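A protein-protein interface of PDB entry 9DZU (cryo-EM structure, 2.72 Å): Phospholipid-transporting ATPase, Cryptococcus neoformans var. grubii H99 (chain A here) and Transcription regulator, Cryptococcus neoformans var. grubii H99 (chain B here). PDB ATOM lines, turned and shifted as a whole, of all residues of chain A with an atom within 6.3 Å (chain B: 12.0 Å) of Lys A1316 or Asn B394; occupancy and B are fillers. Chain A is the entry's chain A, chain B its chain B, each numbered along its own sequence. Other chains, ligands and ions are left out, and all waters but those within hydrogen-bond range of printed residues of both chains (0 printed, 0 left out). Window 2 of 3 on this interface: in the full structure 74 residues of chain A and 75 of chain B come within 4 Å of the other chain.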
ATOM      1  N   HIS A1310      29.430  -7.097 -27.747  1.00  0.00           N
ATOM      2  CA  HIS A1310      28.069  -7.294 -27.280  1.00  0.00           C
ATOM      3  C   HIS A1310      27.778  -6.154 -26.320  1.00  0.00           C
ATOM      4  O   HIS A1310      28.681  -5.739 -25.581  1.00  0.00           O
ATOM      5  CB  HIS A1310      27.881  -8.642 -26.578  1.00  0.00           C
ATOM      6  CG  HIS A1310      26.455  -8.964 -26.258  1.00  0.00           C
ATOM      7  ND1 HIS A1310      25.843  -8.554 -25.093  1.00  0.00           N
ATOM      8  CD2 HIS A1310      25.521  -9.659 -26.948  1.00  0.00           C
ATOM      9  CE1 HIS A1310      24.593  -8.981 -25.081  1.00  0.00           C
ATOM     10  NE2 HIS A1310      24.373  -9.654 -26.195  1.00  0.00           N
ATOM     11  N   PRO A1311      26.550  -5.627 -26.307  1.00  0.00           N
ATOM     12  CA  PRO A1311      26.270  -4.464 -25.447  1.00  0.00           C
ATOM     13  C   PRO A1311      26.558  -4.700 -23.976  1.00  0.00           C
ATOM     14  O   PRO A1311      27.002  -3.775 -23.284  1.00  0.00           O
ATOM     15  CB  PRO A1311      24.781  -4.203 -25.703  1.00  0.00           C
ATOM     16  CG  PRO A1311      24.546  -4.721 -27.075  1.00  0.00           C
ATOM     17  CD  PRO A1311      25.431  -5.925 -27.216  1.00  0.00           C
ATOM     18  N   MET A1312      26.322  -5.911 -23.470  1.00  0.00           N
ATOM     19  CA  MET A1312      26.550  -6.210 -22.064  1.00  0.00           C
ATOM     20  C   MET A1312      27.787  -7.061 -21.815  1.00  0.00           C
ATOM     21  O   MET A1312      28.131  -7.293 -20.652  1.00  0.00           O
ATOM     22  CB  MET A1312      25.329  -6.920 -21.466  1.00  0.00           C
ATOM     23  CG  MET A1312      24.081  -6.066 -21.382  1.00  0.00           C
ATOM     24  SD  MET A1312      22.693  -6.955 -20.648  1.00  0.00           S
ATOM     25  CE  MET A1312      22.462  -8.271 -21.842  1.00  0.00           C
ATOM     26  N   LEU A1313      28.461  -7.532 -22.863  1.00  0.00           N
ATOM     27  CA  LEU A1313      29.614  -8.410 -22.703  1.00  0.00           C
ATOM     28  C   LEU A1313      30.895  -7.795 -23.251  1.00  0.00           C
ATOM     29  O   LEU A1313      31.911  -7.781 -22.550  1.00  0.00           O
ATOM     30  CB  LEU A1313      29.331  -9.758 -23.370  1.00  0.00           C
ATOM     31  CG  LEU A1313      29.813 -10.994 -22.624  1.00  0.00           C
ATOM     32  CD1 LEU A1313      29.539 -10.852 -21.139  1.00  0.00           C
ATOM     33  CD2 LEU A1313      29.114 -12.211 -23.179  1.00  0.00           C
ATOM     34  N   GLY A1314      30.887  -7.300 -24.485  1.00  0.00           N
ATOM     35  CA  GLY A1314      32.099  -6.775 -25.081  1.00  0.00           C
ATOM     36  C   GLY A1314      32.040  -5.303 -25.423  1.00  0.00           C
ATOM     37  O   GLY A1314      33.053  -4.602 -25.335  1.00  0.00           O
ATOM     38  N   GLY A1315      30.857  -4.818 -25.808  1.00  0.00           N
ATOM     39  CA  GLY A1315      30.714  -3.409 -26.130  1.00  0.00           C
ATOM     40  C   GLY A1315      30.889  -2.512 -24.925  1.00  0.00           C
ATOM     41  O   GLY A1315      31.205  -1.328 -25.068  1.00  0.00           O
ATOM     42  N   LYS A1316      30.687  -3.057 -23.727  1.00  0.00           N
ATOM     43  CA  LYS A1316      30.963  -2.340 -22.493  1.00  0.00           C
ATOM     44  C   LYS A1316      32.435  -2.400 -22.106  1.00  0.00           C
ATOM     45  O   LYS A1316      32.842  -1.709 -21.167  1.00  0.00           O
ATOM     46  CB  LYS A1316      30.090  -2.913 -21.369  1.00  0.00           C
ATOM     47  CG  LYS A1316      29.934  -2.019 -20.152  1.00  0.00           C
ATOM     48  CD  LYS A1316      28.902  -2.577 -19.190  1.00  0.00           C
ATOM     49  CE  LYS A1316      27.522  -2.595 -19.821  1.00  0.00           C
ATOM     50  NZ  LYS A1316      26.471  -3.037 -18.866  1.00  0.00           N
ATOM     51  N   LEU A1317      33.235  -3.195 -22.819  1.00  0.00           N
ATOM     52  CA  LEU A1317      34.661  -3.369 -22.539  1.00  0.00           C
ATOM     53  C   LEU A1317      34.883  -3.793 -21.091  1.00  0.00           C
ATOM     54  O   LEU A1317      35.811  -3.342 -20.415  1.00  0.00           O
ATOM     55  CB  LEU A1317      35.451  -2.100 -22.869  1.00  0.00           C
ATOM     56  CG  LEU A1317      35.890  -1.909 -24.323  1.00  0.00           C
ATOM     57  CD1 LEU A1317      36.573  -3.164 -24.838  1.00  0.00           C
ATOM     58  CD2 LEU A1317      34.720  -1.519 -25.216  1.00  0.00           C
ATOM     59  N   ALA A1318      34.016  -4.678 -20.616  1.00  0.00           N
ATOM     60  CA  ALA A1318      34.098  -5.158 -19.245  1.00  0.00           C
ATOM     61  C   ALA A1318      33.562  -6.577 -19.135  1.00  0.00           C
ATOM     62  O   ALA A1318      32.789  -7.024 -19.979  1.00  0.00           O
ATOM     63  CB  ALA A1318      33.341  -4.227 -18.314  1.00  0.00           C
ATOM     64  N   LYS B 384      15.534 -16.646 -15.555  1.00  0.00           N
ATOM     65  CA  LYS B 384      16.021 -16.996 -16.880  1.00  0.00           C
ATOM     66  C   LYS B 384      17.435 -17.553 -16.778  1.00  0.00           C
ATOM     67  O   LYS B 384      18.306 -16.945 -16.151  1.00  0.00           O
ATOM     68  CB  LYS B 384      15.990 -15.780 -17.805  1.00  0.00           C
ATOM     69  CG  LYS B 384      16.563 -14.511 -17.190  1.00  0.00           C
ATOM     70  CD  LYS B 384      16.433 -13.331 -18.142  1.00  0.00           C
ATOM     71  CE  LYS B 384      16.948 -12.047 -17.509  1.00  0.00           C
ATOM     72  NZ  LYS B 384      16.829 -10.883 -18.430  1.00  0.00           N
ATOM     73  N   GLY B 386      21.143 -18.440 -17.955  1.00  0.00           N
ATOM     74  CA  GLY B 386      22.115 -17.795 -18.821  1.00  0.00           C
ATOM     75  C   GLY B 386      21.832 -16.334 -19.090  1.00  0.00           C
ATOM     76  O   GLY B 386      21.970 -15.877 -20.231  1.00  0.00           O
ATOM     77  N   ASP B 387      21.430 -15.589 -18.064  1.00  0.00           N
ATOM     78  CA  ASP B 387      21.223 -14.159 -18.220  1.00  0.00           C
ATOM     79  C   ASP B 387      22.564 -13.436 -18.150  1.00  0.00           C
ATOM     80  O   ASP B 387      23.623 -14.045 -17.991  1.00  0.00           O
ATOM     81  CB  ASP B 387      20.252 -13.639 -17.163  1.00  0.00           C
ATOM     82  CG  ASP B 387      20.620 -14.081 -15.763  1.00  0.00           C
ATOM     83  OD1 ASP B 387      21.615 -14.821 -15.611  1.00  0.00           O
ATOM     84  OD2 ASP B 387      19.911 -13.688 -14.812  1.00  0.00           O
ATOM     85  N   MET B 388      22.525 -12.113 -18.290  1.00  0.00           N
ATOM     86  CA  MET B 388      23.734 -11.308 -18.259  1.00  0.00           C
ATOM     87  C   MET B 388      23.593 -10.047 -17.422  1.00  0.00           C
ATOM     88  O   MET B 388      24.525  -9.237 -17.395  1.00  0.00           O
ATOM     89  CB  MET B 388      24.160 -10.928 -19.685  1.00  0.00           C
ATOM     90  CG  MET B 388      24.571 -12.111 -20.541  1.00  0.00           C
ATOM     91  SD  MET B 388      24.771 -11.686 -22.276  1.00  0.00           S
ATOM     92  CE  MET B 388      26.007 -10.401 -22.161  1.00  0.00           C
ATOM     93  N   SER B 389      22.466  -9.855 -16.742  1.00  0.00           N
ATOM     94  CA  SER B 389      22.258  -8.676 -15.919  1.00  0.00           C
ATOM     95  C   SER B 389      22.780  -8.840 -14.498  1.00  0.00           C
ATOM     96  O   SER B 389      22.809  -7.857 -13.751  1.00  0.00           O
ATOM     97  CB  SER B 389      20.768  -8.319 -15.875  1.00  0.00           C
ATOM     98  OG  SER B 389      20.546  -7.162 -15.087  1.00  0.00           O
ATOM     99  N   LEU B 390      23.185 -10.045 -14.104  1.00  0.00           N
ATOM    100  CA  LEU B 390      23.722 -10.281 -12.771  1.00  0.00           C
ATOM    101  C   LEU B 390      25.233 -10.472 -12.765  1.00  0.00           C
ATOM    102  O   LEU B 390      25.791 -10.879 -11.741  1.00  0.00           O
ATOM    103  CB  LEU B 390      23.029 -11.483 -12.122  1.00  0.00           C
ATOM    104  CG  LEU B 390      22.595 -12.665 -12.988  1.00  0.00           C
ATOM    105  CD1 LEU B 390      23.789 -13.394 -13.575  1.00  0.00           C
ATOM    106  CD2 LEU B 390      21.741 -13.614 -12.167  1.00  0.00           C
ATOM    107  N   LEU B 391      25.905 -10.193 -13.879  1.00  0.00           N
ATOM    108  CA  LEU B 391      27.358 -10.214 -13.898  1.00  0.00           C
ATOM    109  C   LEU B 391      27.911  -9.044 -13.092  1.00  0.00           C
ATOM    110  O   LEU B 391      27.218  -8.063 -12.810  1.00  0.00           O
ATOM    111  CB  LEU B 391      27.879 -10.158 -15.333  1.00  0.00           C
ATOM    112  CG  LEU B 391      27.542 -11.353 -16.222  1.00  0.00           C
ATOM    113  CD1 LEU B 391      27.745 -10.995 -17.680  1.00  0.00           C
ATOM    114  CD2 LEU B 391      28.392 -12.544 -15.849  1.00  0.00           C
ATOM    115  N   SER B 392      29.185  -9.164 -12.713  1.00  0.00           N
ATOM    116  CA  SER B 392      29.798  -8.155 -11.856  1.00  0.00           C
ATOM    117  C   SER B 392      29.841  -6.794 -12.537  1.00  0.00           C
ATOM    118  O   SER B 392      29.525  -5.772 -11.917  1.00  0.00           O
ATOM    119  CB  SER B 392      31.205  -8.598 -11.453  1.00  0.00           C
ATOM    120  OG  SER B 392      31.169  -9.814 -10.729  1.00  0.00           O
ATOM    121  N   TRP B 393      30.225  -6.757 -13.812  1.00  0.00           N
ATOM    122  CA  TRP B 393      30.344  -5.480 -14.503  1.00  0.00           C
ATOM    123  C   TRP B 393      28.992  -4.912 -14.915  1.00  0.00           C
ATOM    124  O   TRP B 393      28.854  -3.690 -15.039  1.00  0.00           O
ATOM    125  CB  TRP B 393      31.262  -5.620 -15.719  1.00  0.00           C
ATOM    126  CG  TRP B 393      30.945  -6.776 -16.613  1.00  0.00           C
ATOM    127  CD1 TRP B 393      30.094  -6.780 -17.672  1.00  0.00           C
ATOM    128  CD2 TRP B 393      31.497  -8.095 -16.537  1.00  0.00           C
ATOM    129  NE1 TRP B 393      30.070  -8.019 -18.257  1.00  0.00           N
ATOM    130  CE2 TRP B 393      30.924  -8.846 -17.578  1.00  0.00           C
ATOM    131  CE3 TRP B 393      32.415  -8.716 -15.686  1.00  0.00           C
ATOM    132  CZ2 TRP B 393      31.240 -10.184 -17.792  1.00  0.00           C
ATOM    133  CZ3 TRP B 393      32.726 -10.044 -15.902  1.00  0.00           C
ATOM    134  CH2 TRP B 393      32.138 -10.762 -16.944  1.00  0.00           C
ATOM    135  N   ASN B 394      27.992  -5.762 -15.130  1.00  0.00           N
ATOM    136  CA  ASN B 394      26.660  -5.303 -15.529  1.00  0.00           C
ATOM    137  C   ASN B 394      25.752  -5.079 -14.324  1.00  0.00           C
ATOM    138  O   ASN B 394      24.626  -5.572 -14.270  1.00  0.00           O
ATOM    139  CB  ASN B 394      26.039  -6.301 -16.499  1.00  0.00           C
ATOM    140  CG  ASN B 394      26.822  -6.426 -17.785  1.00  0.00           C
ATOM    141  OD1 ASN B 394      27.407  -5.456 -18.264  1.00  0.00           O
ATOM    142  ND2 ASN B 394      26.842  -7.626 -18.351  1.00  0.00           N
ATOM    143  N   GLN B 395      26.237  -4.319 -13.347  1.00  0.00           N
ATOM    144  CA  GLN B 395      25.467  -3.972 -12.163  1.00  0.00           C
ATOM    145  C   GLN B 395      25.836  -2.560 -11.740  1.00  0.00           C
ATOM    146  O   GLN B 395      26.946  -2.100 -12.035  1.00  0.00           O
ATOM    147  CB  GLN B 395      25.722  -4.953 -11.010  1.00  0.00           C
ATOM    148  CG  GLN B 395      25.005  -6.283 -11.158  1.00  0.00           C
ATOM    149  CD  GLN B 395      25.202  -7.183  -9.959  1.00  0.00           C
ATOM    150  OE1 GLN B 395      25.951  -6.855  -9.040  1.00  0.00           O
ATOM    151  NE2 GLN B 395      24.526  -8.326  -9.960  1.00  0.00           N
ATOM    152  N   PRO B 396      24.934  -1.846 -11.066  1.00  0.00           N
ATOM    153  CA  PRO B 396      25.267  -0.495 -10.600  1.00  0.00           C
ATOM    154  C   PRO B 396      26.409  -0.519  -9.595  1.00  0.00           C
ATOM    155  O   PRO B 396      26.559  -1.467  -8.820  1.00  0.00           O
ATOM    156  CB  PRO B 396      23.962  -0.010  -9.958  1.00  0.00           C
ATOM    157  CG  PRO B 396      22.896  -0.847 -10.582  1.00  0.00           C
ATOM    158  CD  PRO B 396      23.525  -2.186 -10.808  1.00  0.00           C
ATOM    159  N   ASN B 397      27.215   0.540  -9.621  1.00  0.00           N
ATOM    160  CA  ASN B 397      28.369   0.686  -8.736  1.00  0.00           C
ATOM    161  C   ASN B 397      29.327  -0.495  -8.863  1.00  0.00           C
ATOM    162  O   ASN B 397      29.550  -1.009  -9.959  1.00  0.00           O
ATOM    163  CB  ASN B 397      27.919   0.844  -7.280  1.00  0.00           C
ATOM    164  CG  ASN B 397      29.084   0.970  -6.318  1.00  0.00           C
ATOM    165  OD1 ASN B 397      29.564  -0.024  -5.772  1.00  0.00           O
ATOM    166  ND2 ASN B 397      29.547   2.196  -6.106  1.00  0.00           N
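Hydrophobic or aromatic side chains of chain A that line the printed part of chain B: His A1310, Met A1312, Leu A1313 and Ala A1318. Hydrophobic or aromatic side chains of chain B within 4 Å of the printed part of chain A: Met B388, Leu B391 and Trp B393. Along chain B the printed residues that touch a printed residue of chain A span positions 388 to 394.
O of Met B388 is in hydrogen-bond range of ND2 of Asn B394, at 3.0 Å. ND2 of Asn B394 lies close to NE1 of Trp B393, 3.3 Å away. A ring nitrogen (ND1) of His A1310 sits at hydrogen-bond distance from the backbone NH (N) of Met A1312.
His A1310 touches Met B388 (ND1 to CE, 3.5 Å). CB of Met A1312 touches CE of Met B388 (3.6 Å). CE of Met B388 touches CB of Leu A1313, 3.6 Å away. Leu B391 touches Leu A1313 (CD1 to CD1, 3.9 Å). CD1 of Leu A1313 touches CZ2 of Trp B393, 3.8 Å away.
O of Met A1312 sits at hydrogen-bond distance from NE1 of Trp B393, 3.2 Å away. O of Ala A1318 is in hydrogen-bond range of NE1 of Trp B393, at 3.4 Å. The backbone carbonyl oxygen of Met A1312 sits at hydrogen-bond distance from the side-chain amide nitrogen of Asn B394, 2.7 Å away. OD1 of Asn B394 is in hydrogen-bond range of NZ of Lys A1316, 2.7 Å away.
Of the printed residues of chain A, Asn B394 touches Met A1312 and Lys A1316. No residue of chain B comes within 4 Å of Pro A1311. Met A1312 touches just these residues of chain B: Met B388 (3.6 Å), Trp B393 (3.2 Å) and Asn B394 (2.7 Å). Of chain B, only Met B388 (3.6 Å), Leu B391 (3.9 Å) and Trp B393 (3.8 Å) come within 4 Å of Leu A1313. No residue of chain B comes within 4 Å of Gly A1315. Ala A1318 touches just one residue of chain B: Trp B393 (3.4 Å). Printed residues of chain B within 4 Å of His A1310: Met B388 (3.5 Å). Of the printed residues of chain A, Leu B391 touches Leu A1313 (3.9 Å). Of the printed residues of chain A, Met B388 touches His A1310 (3.5 Å), Met A1312 (3.6 Å) and Leu A1313 (3.6 Å). Printed residues of chain A within 4 Å of Trp B393: Met A1312, Leu A1313 and Ala A1318. Gly B386 touches none of the printed residues of chain A. Gln B395 touches none of the printed residues of chain A. The nearest residue of chain B that does not touch Lys A1316 is Trp B393 (4.3 Å). The nearest residue of chain A that does not touch Asn B394 is Leu A1313 (4.8 Å).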
